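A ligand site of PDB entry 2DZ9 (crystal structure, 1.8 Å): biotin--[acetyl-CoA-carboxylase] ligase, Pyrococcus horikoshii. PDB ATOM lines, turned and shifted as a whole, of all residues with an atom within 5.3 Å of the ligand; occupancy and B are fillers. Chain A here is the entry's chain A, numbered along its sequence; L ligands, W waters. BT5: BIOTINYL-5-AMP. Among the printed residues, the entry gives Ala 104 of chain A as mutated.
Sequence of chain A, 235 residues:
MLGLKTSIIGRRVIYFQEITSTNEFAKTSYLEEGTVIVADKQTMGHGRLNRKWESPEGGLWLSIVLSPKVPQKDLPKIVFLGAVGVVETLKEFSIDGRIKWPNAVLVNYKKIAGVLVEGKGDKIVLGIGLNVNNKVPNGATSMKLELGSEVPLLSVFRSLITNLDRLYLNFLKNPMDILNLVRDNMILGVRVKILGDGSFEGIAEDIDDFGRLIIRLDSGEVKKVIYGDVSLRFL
NH1 of Arg 51 is in salt-bridge range of OP2 of the ligand (3.1 Å). OG1 of Thr 22 sits at hydrogen-bond distance from N1B of the ligand, at 3.1 Å. The side-chain amino group (NZ) of Lys 111 lies within salt-bridge range of an oxygen (OP1) of the ligand, 3.3 Å away. N6 of the ligand sits at hydrogen-bond distance from O of Glu 54 (2.9 Å). The guanidinium group of Arg 48 is in salt-bridge range of an oxygen (OP2) of the ligand (3.98 Å). N7 of the ligand lies within hydrogen-bond range of N of Glu 54 (3.0 Å). The backbone NH of His 46 sits at hydrogen-bond distance from an oxygen (O3B) of the ligand (3.0 Å). ND2 of Asn 131 sits at hydrogen-bond distance from N1 of the ligand, at 2.8 Å. A nitrogen (N2B) of the ligand lies within hydrogen-bond range of the backbone carbonyl oxygen (O) of His 46. The side-chain hydroxyl (OG) of Ser 21 sits at hydrogen-bond distance from an oxygen (O3B) of the ligand (2.6 Å). OP2 of the ligand sits at hydrogen-bond distance from N of Arg 48, at 3.2 Å. The side-chain amide oxygen of Gln 42 lies within hydrogen-bond range of a nitrogen (N1B) of the ligand (3.0 Å).
The side-chain hydroxyl (OG) of Ser 21 sits close to the backbone NH (N) of Asn 23 (3.3 Å). The backbone NH (N) of Asn 131 lies within hydrogen-bond range of the backbone carbonyl oxygen (O) of Ile 112 (2.9 Å). The backbone NH of Gly 127 sits close to the side-chain amide oxygen of Asn 23 (3.5 Å). O of Leu 62 lies within hydrogen-bond range of N of Ile 128 (2.8 Å). O of Asn 103 lies within hydrogen-bond range of N of Val 115 (2.7 Å). NE2 of Gln 42 is in hydrogen-bond range of OG of Ser 55, at 2.9 Å. The backbone carbonyl oxygen of Leu 116 is in hydrogen-bond range of the backbone NH of Gly 127 (2.8 Å). The side-chain amide nitrogen (ND2) of Asn 23 is in hydrogen-bond range of the backbone carbonyl oxygen (O) of Leu 116, 3.3 Å away.
The backbone carbonyl oxygen (O) of Ile 128 sits close to a sulfur (S1B) of the ligand, at 3.7 Å. Merely in contact with the ligand: Asn 23, Gly 45, Gly 47, Lys 52, Trp 53, Leu 62, Ser 63, Asn 103, Gly 114, Val 115, Leu 116, Gly 129, Pro 137 and Ala 140. Hydrophobic or aromatic side chains within 4 Å of the ligand: His 46, Trp 53, Leu 116, Pro 137 and Ala 140. 24 residues have an atom within 4 Å of the ligand: Ser 21, Thr 22, Asn 23, Gln 42, Gly 45, His 46, Gly 47, Arg 48, Arg 51, Lys 52, Trp 53, Glu 54, Leu 62, Ser 63, Asn 103, Lys 111, Gly 114, Val 115, Leu 116, Ile 128, Gly 129, Asn 131, Pro 137 and Ala 140.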
ATOM      1  N   SER A  21      -6.718  17.525 -23.862  1.00  0.00           N
ATOM      2  CA  SER A  21      -6.016  16.310 -24.262  1.00  0.00           C
ATOM      3  C   SER A  21      -4.862  16.672 -25.177  1.00  0.00           C
ATOM      4  O   SER A  21      -5.051  17.378 -26.164  1.00  0.00           O
ATOM      5  CB  SER A  21      -6.969  15.360 -25.004  1.00  0.00           C
ATOM      6  OG  SER A  21      -6.260  14.329 -25.675  1.00  0.00           O
ATOM      7  N   THR A  22      -3.652  16.198 -24.858  1.00  0.00           N
ATOM      8  CA  THR A  22      -2.498  16.496 -25.694  1.00  0.00           C
ATOM      9  C   THR A  22      -2.662  15.867 -27.081  1.00  0.00           C
ATOM     10  O   THR A  22      -2.218  16.431 -28.088  1.00  0.00           O
ATOM     11  CB  THR A  22      -1.177  16.005 -25.035  1.00  0.00           C
ATOM     12  OG1 THR A  22      -1.248  14.584 -24.803  1.00  0.00           O
ATOM     13  CG2 THR A  22      -0.952  16.712 -23.719  1.00  0.00           C
ATOM     14  N   ASN A  23      -3.302  14.702 -27.135  1.00  0.00           N
ATOM     15  CA  ASN A  23      -3.527  14.037 -28.417  1.00  0.00           C
ATOM     16  C   ASN A  23      -4.468  14.849 -29.294  1.00  0.00           C
ATOM     17  O   ASN A  23      -4.217  15.035 -30.486  1.00  0.00           O
ATOM     18  CB  ASN A  23      -4.096  12.635 -28.200  1.00  0.00           C
ATOM     19  CG  ASN A  23      -3.093  11.548 -28.495  1.00  0.00           C
ATOM     20  OD1 ASN A  23      -1.912  11.676 -28.184  1.00  0.00           O
ATOM     21  ND2 ASN A  23      -3.550  10.459 -29.095  1.00  0.00           N
ATOM     22  N   GLN A  42      -4.539  16.708 -17.667  1.00  0.00           N
ATOM     23  CA  GLN A  42      -5.518  16.720 -18.740  1.00  0.00           C
ATOM     24  C   GLN A  42      -6.924  16.621 -18.132  1.00  0.00           C
ATOM     25  O   GLN A  42      -7.172  15.869 -17.209  1.00  0.00           O
ATOM     26  CB  GLN A  42      -5.269  15.510 -19.671  1.00  0.00           C
ATOM     27  CG  GLN A  42      -3.827  15.380 -20.171  1.00  0.00           C
ATOM     28  CD  GLN A  42      -3.778  14.348 -21.281  1.00  0.00           C
ATOM     29  OE1 GLN A  42      -3.608  14.630 -22.457  1.00  0.00           O
ATOM     30  NE2 GLN A  42      -3.843  13.073 -20.838  1.00  0.00           N
ATOM     31  N   MET A  44      -9.579  16.025 -20.106  1.00  0.00           N
ATOM     32  CA  MET A  44     -10.289  15.057 -20.933  1.00  0.00           C
ATOM     33  C   MET A  44      -9.315  14.062 -21.588  1.00  0.00           C
ATOM     34  O   MET A  44      -9.370  13.814 -22.788  1.00  0.00           O
ATOM     35  CB  MET A  44     -11.033  15.808 -22.031  1.00  0.00           C
ATOM     36  CG  MET A  44     -12.082  16.798 -21.510  1.00  0.00           C
ATOM     37  SD  MET A  44     -12.892  17.694 -22.843  1.00  0.00           S
ATOM     38  CE  MET A  44     -14.083  16.415 -23.267  1.00  0.00           C
ATOM     39  N   GLY A  45      -8.413  13.486 -20.807  1.00  0.00           N
ATOM     40  CA  GLY A  45      -7.491  12.521 -21.368  1.00  0.00           C
ATOM     41  C   GLY A  45      -8.274  11.276 -21.747  1.00  0.00           C
ATOM     42  O   GLY A  45      -9.261  10.927 -21.105  1.00  0.00           O
ATOM     43  N   HIS A  46      -7.851  10.609 -22.817  1.00  0.00           N
ATOM     44  CA  HIS A  46      -8.565   9.409 -23.220  1.00  0.00           C
ATOM     45  C   HIS A  46      -7.679   8.331 -23.818  1.00  0.00           C
ATOM     46  O   HIS A  46      -6.544   8.581 -24.224  1.00  0.00           O
ATOM     47  CB  HIS A  46      -9.671   9.776 -24.220  1.00  0.00           C
ATOM     48  CG  HIS A  46      -9.169  10.338 -25.511  1.00  0.00           C
ATOM     49  ND1 HIS A  46      -8.694   9.535 -26.532  1.00  0.00           N
ATOM     50  CD2 HIS A  46      -9.051  11.605 -25.945  1.00  0.00           C
ATOM     51  CE1 HIS A  46      -8.307  10.299 -27.542  1.00  0.00           C
ATOM     52  NE2 HIS A  46      -8.518  11.565 -27.210  1.00  0.00           N
ATOM     53  N   GLY A  47      -8.219   7.116 -23.834  1.00  0.00           N
ATOM     54  CA  GLY A  47      -7.509   5.979 -24.402  1.00  0.00           C
ATOM     55  C   GLY A  47      -8.300   5.566 -25.626  1.00  0.00           C
ATOM     56  O   GLY A  47      -8.926   6.402 -26.266  1.00  0.00           O
ATOM     57  N   ARG A  48      -8.283   4.274 -25.944  1.00  0.00           N
ATOM     58  CA  ARG A  48      -9.015   3.777 -27.104  1.00  0.00           C
ATOM     59  C   ARG A  48     -10.525   3.895 -26.873  1.00  0.00           C
ATOM     60  O   ARG A  48     -10.984   3.915 -25.736  1.00  0.00           O
ATOM     61  CB  ARG A  48      -8.626   2.314 -27.353  1.00  0.00           C
ATOM     62  CG  ARG A  48      -7.129   2.076 -27.327  1.00  0.00           C
ATOM     63  CD  ARG A  48      -6.752   0.632 -27.616  1.00  0.00           C
ATOM     64  NE  ARG A  48      -7.810  -0.104 -28.307  1.00  0.00           N
ATOM     65  CZ  ARG A  48      -8.633  -0.966 -27.721  1.00  0.00           C
ATOM     66  NH1 ARG A  48      -8.529  -1.210 -26.420  1.00  0.00           N
ATOM     67  NH2 ARG A  48      -9.558  -1.599 -28.437  1.00  0.00           N
ATOM     68  N   ARG A  51     -12.161   6.013 -24.118  1.00  0.00           N
ATOM     69  CA  ARG A  51     -12.180   5.589 -22.721  1.00  0.00           C
ATOM     70  C   ARG A  51     -11.451   6.667 -21.918  1.00  0.00           C
ATOM     71  O   ARG A  51     -10.486   7.257 -22.395  1.00  0.00           O
ATOM     72  CB  ARG A  51     -11.452   4.255 -22.555  1.00  0.00           C
ATOM     73  CG  ARG A  51     -12.153   3.061 -23.200  1.00  0.00           C
ATOM     74  CD  ARG A  51     -11.239   1.858 -23.243  1.00  0.00           C
ATOM     75  NE  ARG A  51     -11.840   0.748 -23.978  1.00  0.00           N
ATOM     76  CZ  ARG A  51     -11.173  -0.342 -24.342  1.00  0.00           C
ATOM     77  NH1 ARG A  51      -9.881  -0.456 -24.064  1.00  0.00           N
ATOM     78  NH2 ARG A  51     -11.802  -1.305 -25.000  1.00  0.00           N
ATOM     79  N   LYS A  52     -11.899   6.925 -20.697  1.00  0.00           N
ATOM     80  CA  LYS A  52     -11.274   7.947 -19.864  1.00  0.00           C
ATOM     81  C   LYS A  52      -9.873   7.543 -19.384  1.00  0.00           C
ATOM     82  O   LYS A  52      -9.662   6.413 -18.943  1.00  0.00           O
ATOM     83  CB  LYS A  52     -12.160   8.253 -18.651  1.00  0.00           C
ATOM     84  CG  LYS A  52     -11.518   9.115 -17.564  1.00  0.00           C
ATOM     85  CD  LYS A  52     -12.071  10.531 -17.615  1.00  0.00           C
ATOM     86  CE  LYS A  52     -11.257  11.478 -16.757  1.00  0.00           C
ATOM     87  NZ  LYS A  52     -11.458  12.895 -17.150  1.00  0.00           N
ATOM     88  N   TRP A  53      -8.927   8.477 -19.495  1.00  0.00           N
ATOM     89  CA  TRP A  53      -7.561   8.254 -19.027  1.00  0.00           C
ATOM     90  C   TRP A  53      -7.304   9.285 -17.937  1.00  0.00           C
ATOM     91  O   TRP A  53      -7.242  10.496 -18.219  1.00  0.00           O
ATOM     92  CB  TRP A  53      -6.546   8.416 -20.165  1.00  0.00           C
ATOM     93  CG  TRP A  53      -5.127   8.171 -19.704  1.00  0.00           C
ATOM     94  CD1 TRP A  53      -4.223   9.105 -19.299  1.00  0.00           C
ATOM     95  CD2 TRP A  53      -4.483   6.897 -19.544  1.00  0.00           C
ATOM     96  NE1 TRP A  53      -3.065   8.489 -18.879  1.00  0.00           N
ATOM     97  CE2 TRP A  53      -3.195   7.135 -19.026  1.00  0.00           C
ATOM     98  CE3 TRP A  53      -4.884   5.577 -19.789  1.00  0.00           C
ATOM     99  CZ2 TRP A  53      -2.300   6.104 -18.737  1.00  0.00           C
ATOM    100  CZ3 TRP A  53      -3.986   4.539 -19.513  1.00  0.00           C
ATOM    101  CH2 TRP A  53      -2.711   4.818 -18.988  1.00  0.00           C
ATOM    102  N   GLU A  54      -7.189   8.828 -16.694  1.00  0.00           N
ATOM    103  CA  GLU A  54      -6.958   9.727 -15.561  1.00  0.00           C
ATOM    104  C   GLU A  54      -5.594  10.404 -15.724  1.00  0.00           C
ATOM    105  O   GLU A  54      -4.571   9.721 -15.818  1.00  0.00           O
ATOM    106  CB  GLU A  54      -6.992   8.930 -14.255  1.00  0.00           C
ATOM    107  CG  GLU A  54      -8.291   8.141 -14.069  1.00  0.00           C
ATOM    108  CD  GLU A  54      -9.502   9.034 -13.952  1.00  0.00           C
ATOM    109  OE1 GLU A  54      -9.340  10.263 -13.818  1.00  0.00           O
ATOM    110  OE2 GLU A  54     -10.642   8.500 -13.987  1.00  0.00           O
ATOM    111  N   SER A  55      -5.588  11.732 -15.720  1.00  0.00           N
ATOM    112  CA  SER A  55      -4.359  12.490 -15.923  1.00  0.00           C
ATOM    113  C   SER A  55      -4.153  13.613 -14.915  1.00  0.00           C
ATOM    114  O   SER A  55      -4.114  14.784 -15.298  1.00  0.00           O
ATOM    115  CB  SER A  55      -4.352  13.075 -17.341  1.00  0.00           C
ATOM    116  OG  SER A  55      -4.857  12.141 -18.283  1.00  0.00           O
ATOM    117  N   TRP A  61       2.102  13.248 -19.275  1.00  0.00           N
ATOM    118  CA  TRP A  61       1.067  13.190 -20.314  1.00  0.00           C
ATOM    119  C   TRP A  61       1.568  13.966 -21.535  1.00  0.00           C
ATOM    120  O   TRP A  61       1.662  15.193 -21.484  1.00  0.00           O
ATOM    121  CB  TRP A  61      -0.219  13.834 -19.790  1.00  0.00           C
ATOM    122  CG  TRP A  61      -0.492  13.612 -18.324  1.00  0.00           C
ATOM    123  CD1 TRP A  61      -0.692  14.579 -17.375  1.00  0.00           C
ATOM    124  CD2 TRP A  61      -0.602  12.348 -17.640  1.00  0.00           C
ATOM    125  NE1 TRP A  61      -0.925  13.996 -16.144  1.00  0.00           N
ATOM    126  CE2 TRP A  61      -0.872  12.632 -16.278  1.00  0.00           C
ATOM    127  CE3 TRP A  61      -0.498  11.016 -18.047  1.00  0.00           C
ATOM    128  CZ2 TRP A  61      -1.038  11.620 -15.319  1.00  0.00           C
ATOM    129  CZ3 TRP A  61      -0.670  10.011 -17.092  1.00  0.00           C
ATOM    130  CH2 TRP A  61      -0.930  10.325 -15.745  1.00  0.00           C
ATOM    131  N   LEU A  62       1.899  13.265 -22.618  1.00  0.00           N
ATOM    132  CA  LEU A  62       2.400  13.956 -23.808  1.00  0.00           C
ATOM    133  C   LEU A  62       2.035  13.307 -25.145  1.00  0.00           C
ATOM    134  O   LEU A  62       1.658  12.143 -25.188  1.00  0.00           O
ATOM    135  CB  LEU A  62       3.931  14.108 -23.712  1.00  0.00           C
ATOM    136  CG  LEU A  62       4.804  12.843 -23.647  1.00  0.00           C
ATOM    137  CD1 LEU A  62       5.014  12.258 -25.036  1.00  0.00           C
ATOM    138  CD2 LEU A  62       6.152  13.211 -23.037  1.00  0.00           C
ATOM    139  N   SER A  63       2.158  14.091 -26.219  1.00  0.00           N
ATOM    140  CA  SER A  63       1.861  13.609 -27.566  1.00  0.00           C
ATOM    141  C   SER A  63       2.953  14.155 -28.477  1.00  0.00           C
ATOM    142  O   SER A  63       3.429  15.270 -28.296  1.00  0.00           O
ATOM    143  CB  SER A  63       0.504  14.118 -28.045  1.00  0.00           C
ATOM    144  OG  SER A  63      -0.550  13.699 -27.179  1.00  0.00           O
ATOM    145  N   ASN A 103      -0.267  -1.795 -26.723  1.00  0.00           N
ATOM    146  CA  ASN A 103      -0.108  -0.371 -26.367  1.00  0.00           C
ATOM    147  C   ASN A 103       0.040  -0.078 -24.867  1.00  0.00           C
ATOM    148  O   ASN A 103      -0.087   1.065 -24.451  1.00  0.00           O
ATOM    149  CB  ASN A 103      -1.316   0.387 -26.906  1.00  0.00           C
ATOM    150  CG  ASN A 103      -2.553   0.063 -26.085  1.00  0.00           C
ATOM    151  OD1 ASN A 103      -2.807  -1.095 -25.732  1.00  0.00           O
ATOM    152  ND2 ASN A 103      -3.352   1.099 -25.833  1.00  0.00           N
ATOM    153  N   ALA A 104       0.292  -1.084 -24.027  1.00  0.00           N
ATOM    154  CA  ALA A 104       0.415  -0.824 -22.599  1.00  0.00           C
ATOM    155  C   ALA A 104       1.688  -1.380 -21.982  1.00  0.00           C
ATOM    156  O   ALA A 104       2.255  -2.350 -22.475  1.00  0.00           O
ATOM    157  CB  ALA A 104      -0.800  -1.396 -21.872  1.00  0.00           C
ATOM    158  N   LYS A 111      -0.856  -1.693 -14.630  1.00  0.00           N
ATOM    159  CA  LYS A 111      -0.627  -0.731 -15.703  1.00  0.00           C
ATOM    160  C   LYS A 111       0.015   0.567 -15.233  1.00  0.00           C
ATOM    161  O   LYS A 111      -0.544   1.292 -14.406  1.00  0.00           O
ATOM    162  CB  LYS A 111      -1.950  -0.448 -16.420  1.00  0.00           C
ATOM    163  CG  LYS A 111      -1.794   0.295 -17.737  1.00  0.00           C
ATOM    164  CD  LYS A 111      -3.123   0.364 -18.458  1.00  0.00           C
ATOM    165  CE  LYS A 111      -2.985   1.054 -19.801  1.00  0.00           C
ATOM    166  NZ  LYS A 111      -4.250   0.938 -20.566  1.00  0.00           N
ATOM    167  N   ILE A 112       1.203   0.859 -15.765  1.00  0.00           N
ATOM    168  CA  ILE A 112       1.927   2.074 -15.392  1.00  0.00           C
ATOM    169  C   ILE A 112       1.931   3.098 -16.543  1.00  0.00           C
ATOM    170  O   ILE A 112       2.215   4.281 -16.334  1.00  0.00           O
ATOM    171  CB  ILE A 112       3.400   1.722 -14.990  1.00  0.00           C
ATOM    172  CG1 ILE A 112       4.037   2.894 -14.240  1.00  0.00           C
ATOM    173  CG2 ILE A 112       4.233   1.409 -16.230  1.00  0.00           C
ATOM    174  CD1 ILE A 112       5.385   2.549 -13.607  1.00  0.00           C
ATOM    175  N   ALA A 113       1.592   2.633 -17.743  1.00  0.00           N
ATOM    176  CA  ALA A 113       1.562   3.509 -18.919  1.00  0.00           C
ATOM    177  C   ALA A 113       0.742   2.950 -20.075  1.00  0.00           C
ATOM    178  O   ALA A 113       0.635   1.734 -20.253  1.00  0.00           O
ATOM    179  CB  ALA A 113       2.995   3.792 -19.390  1.00  0.00           C
ATOM    180  N   GLY A 114       0.160   3.862 -20.848  1.00  0.00           N
ATOM    181  CA  GLY A 114      -0.631   3.485 -22.008  1.00  0.00           C
ATOM    182  C   GLY A 114      -0.222   4.357 -23.183  1.00  0.00           C
ATOM    183  O   GLY A 114       0.158   5.517 -22.994  1.00  0.00           O
ATOM    184  N   VAL A 115      -0.304   3.805 -24.393  1.00  0.00           N
ATOM    185  CA  VAL A 115       0.065   4.506 -25.614  1.00  0.00           C
ATOM    186  C   VAL A 115      -1.139   4.561 -26.553  1.00  0.00           C
ATOM    187  O   VAL A 115      -1.861   3.576 -26.723  1.00  0.00           O
ATOM    188  CB  VAL A 115       1.237   3.788 -26.334  1.00  0.00           C
ATOM    189  CG1 VAL A 115       1.696   4.573 -27.555  1.00  0.00           C
ATOM    190  CG2 VAL A 115       2.399   3.599 -25.355  1.00  0.00           C
ATOM    191  N   LEU A 116      -1.351   5.718 -27.176  1.00  0.00           N
ATOM    192  CA  LEU A 116      -2.467   5.885 -28.098  1.00  0.00           C
ATOM    193  C   LEU A 116      -2.015   6.626 -29.346  1.00  0.00           C
ATOM    194  O   LEU A 116      -1.585   7.777 -29.264  1.00  0.00           O
ATOM    195  CB  LEU A 116      -3.596   6.673 -27.440  1.00  0.00           C
ATOM    196  CG  LEU A 116      -4.792   6.979 -28.353  1.00  0.00           C
ATOM    197  CD1 LEU A 116      -5.508   5.686 -28.712  1.00  0.00           C
ATOM    198  CD2 LEU A 116      -5.742   7.935 -27.636  1.00  0.00           C
ATOM    199  N   GLY A 127       0.643   9.406 -28.718  1.00  0.00           N
ATOM    200  CA  GLY A 127       0.332   9.813 -27.353  1.00  0.00           C
ATOM    201  C   GLY A 127       0.835   8.822 -26.314  1.00  0.00           C
ATOM    202  O   GLY A 127       0.744   7.609 -26.489  1.00  0.00           O
ATOM    203  N   ILE A 128       1.380   9.357 -25.224  1.00  0.00           N
ATOM    204  CA  ILE A 128       1.912   8.519 -24.165  1.00  0.00           C
ATOM    205  C   ILE A 128       1.512   9.043 -22.790  1.00  0.00           C
ATOM    206  O   ILE A 128       1.708  10.222 -22.485  1.00  0.00           O
ATOM    207  CB  ILE A 128       3.444   8.456 -24.238  1.00  0.00           C
ATOM    208  CG1 ILE A 128       3.871   7.901 -25.604  1.00  0.00           C
ATOM    209  CG2 ILE A 128       3.976   7.576 -23.113  1.00  0.00           C
ATOM    210  CD1 ILE A 128       5.368   7.980 -25.851  1.00  0.00           C
ATOM    211  N   GLY A 129       0.927   8.172 -21.979  1.00  0.00           N
ATOM    212  CA  GLY A 129       0.531   8.532 -20.635  1.00  0.00           C
ATOM    213  C   GLY A 129       1.291   7.617 -19.697  1.00  0.00           C
ATOM    214  O   GLY A 129       1.152   6.399 -19.765  1.00  0.00           O
ATOM    215  N   ASN A 131       2.346   7.076 -15.531  1.00  0.00           N
ATOM    216  CA  ASN A 131       2.140   7.469 -14.148  1.00  0.00           C
ATOM    217  C   ASN A 131       3.480   7.609 -13.419  1.00  0.00           C
ATOM    218  O   ASN A 131       4.257   6.659 -13.325  1.00  0.00           O
ATOM    219  CB  ASN A 131       1.280   6.446 -13.405  1.00  0.00           C
ATOM    220  CG  ASN A 131      -0.103   6.287 -14.010  1.00  0.00           C
ATOM    221  OD1 ASN A 131      -0.789   7.276 -14.278  1.00  0.00           O
ATOM    222  ND2 ASN A 131      -0.514   5.044 -14.227  1.00  0.00           N
ATOM    223  N   ASN A 134       1.690  10.893  -9.700  1.00  0.00           N
ATOM    224  CA  ASN A 134       0.251  11.056  -9.534  1.00  0.00           C
ATOM    225  C   ASN A 134      -0.421   9.865  -8.880  1.00  0.00           C
ATOM    226  O   ASN A 134       0.122   8.762  -8.843  1.00  0.00           O
ATOM    227  CB  ASN A 134      -0.398  11.289 -10.889  1.00  0.00           C
ATOM    228  CG  ASN A 134      -0.060  10.211 -11.897  1.00  0.00           C
ATOM    229  OD1 ASN A 134       1.085  10.113 -12.351  1.00  0.00           O
ATOM    230  ND2 ASN A 134      -1.046   9.381 -12.257  1.00  0.00           N
ATOM    231  N   VAL A 136      -3.149   6.974  -8.879  1.00  0.00           N
ATOM    232  CA  VAL A 136      -3.628   6.184 -10.006  1.00  0.00           C
ATOM    233  C   VAL A 136      -4.891   5.402  -9.698  1.00  0.00           C
ATOM    234  O   VAL A 136      -5.236   5.174  -8.548  1.00  0.00           O
ATOM    235  CB  VAL A 136      -2.545   5.185 -10.480  1.00  0.00           C
ATOM    236  CG1 VAL A 136      -1.284   5.937 -10.881  1.00  0.00           C
ATOM    237  CG2 VAL A 136      -2.236   4.196  -9.351  1.00  0.00           C
ATOM    238  N   PRO A 137      -5.620   4.985 -10.744  1.00  0.00           N
ATOM    239  CA  PRO A 137      -6.856   4.219 -10.564  1.00  0.00           C
ATOM    240  C   PRO A 137      -6.561   2.764 -10.208  1.00  0.00           C
ATOM    241  O   PRO A 137      -5.402   2.330 -10.191  1.00  0.00           O
ATOM    242  CB  PRO A 137      -7.564   4.380 -11.901  1.00  0.00           C
ATOM    243  CG  PRO A 137      -6.429   4.475 -12.869  1.00  0.00           C
ATOM    244  CD  PRO A 137      -5.444   5.365 -12.159  1.00  0.00           C
ATOM    245  N   ALA A 140      -3.739  -0.041 -11.509  1.00  0.00           N
ATOM    246  CA  ALA A 140      -2.599   0.694 -12.048  1.00  0.00           C
ATOM    247  C   ALA A 140      -1.508   0.846 -10.998  1.00  0.00           C
ATOM    248  O   ALA A 140      -1.672   0.457  -9.842  1.00  0.00           O
ATOM    249  CB  ALA A 140      -3.058   2.075 -12.522  1.00  0.00           C
HETATM  250  CBB BT5 L   1      -4.534   3.484 -23.270  1.00  0.00           C
HETATM  251  OBB BT5 L   1      -5.739   3.188 -23.583  1.00  0.00           O
HETATM  252  OCB BT5 L   1      -3.827   2.709 -22.568  1.00  0.00           O
HETATM  253  CAB BT5 L   1      -4.000   4.821 -23.801  1.00  0.00           C
HETATM  254  C9B BT5 L   1      -3.779   5.851 -23.062  1.00  0.00           C
HETATM  255  C8B BT5 L   1      -3.078   6.981 -23.765  1.00  0.00           C
HETATM  256  C7B BT5 L   1      -2.876   8.146 -22.800  1.00  0.00           C
HETATM  257  C2B BT5 L   1      -2.181   9.377 -23.353  1.00  0.00           C
HETATM  258  S1B BT5 L   1      -1.995  10.678 -22.143  1.00  0.00           S
HETATM  259  C6B BT5 L   1      -1.249  11.679 -23.447  1.00  0.00           C
HETATM  260  C5B BT5 L   1      -2.271  11.507 -24.600  1.00  0.00           C
HETATM  261  N1B BT5 L   1      -3.437  12.413 -24.479  1.00  0.00           N
HETATM  262  C3B BT5 L   1      -4.565  11.682 -24.398  1.00  0.00           C
HETATM  263  O3B BT5 L   1      -5.737  12.166 -24.280  1.00  0.00           O
HETATM  264  N2B BT5 L   1      -4.298  10.340 -24.456  1.00  0.00           N
HETATM  265  C4B BT5 L   1      -2.872  10.098 -24.588  1.00  0.00           C
HETATM  266  P   BT5 L   1      -6.627   1.787 -23.174  1.00  0.00           P
HETATM  267  OP1 BT5 L   1      -5.853   0.512 -23.438  1.00  0.00           O
HETATM  268  OP2 BT5 L   1      -7.742   1.848 -23.993  1.00  0.00           O
HETATM  269  O5' BT5 L   1      -6.842   1.815 -21.761  1.00  0.00           O
HETATM  270  C5' BT5 L   1      -7.536   2.806 -20.980  1.00  0.00           C
HETATM  271  C4' BT5 L   1      -7.791   2.149 -19.737  1.00  0.00           C
HETATM  272  O4' BT5 L   1      -6.784   2.275 -18.760  1.00  0.00           O
HETATM  273  C3' BT5 L   1      -9.039   2.706 -19.129  1.00  0.00           C
HETATM  274  O3' BT5 L   1     -10.234   2.103 -19.656  1.00  0.00           O
HETATM  275  C2' BT5 L   1      -8.835   2.507 -17.634  1.00  0.00           C
HETATM  276  O2' BT5 L   1      -9.424   1.311 -17.139  1.00  0.00           O
HETATM  277  C1' BT5 L   1      -7.334   2.499 -17.446  1.00  0.00           C
HETATM  278  N9  BT5 L   1      -6.698   3.818 -16.964  1.00  0.00           N
HETATM  279  C8  BT5 L   1      -7.250   5.106 -16.958  1.00  0.00           C
HETATM  280  N7  BT5 L   1      -6.340   5.999 -16.453  1.00  0.00           N
HETATM  281  C5  BT5 L   1      -5.228   5.290 -16.133  1.00  0.00           C
HETATM  282  C6  BT5 L   1      -4.000   5.705 -15.582  1.00  0.00           C
HETATM  283  N6  BT5 L   1      -3.787   6.986 -15.288  1.00  0.00           N
HETATM  284  N1  BT5 L   1      -3.008   4.707 -15.363  1.00  0.00           N
HETATM  285  C2  BT5 L   1      -3.210   3.350 -15.668  1.00  0.00           C
HETATM  286  N3  BT5 L   1      -4.451   2.940 -16.217  1.00  0.00           N
HETATM  287  C4  BT5 L   1      -5.437   3.916 -16.448  1.00  0.00           C
HETATM  288  O   HOH W   1      -5.219   0.248 -15.167  1.00  0.00           O
HETATM  289  O   HOH W   2     -10.652  -0.697 -19.921  1.00  0.00           O
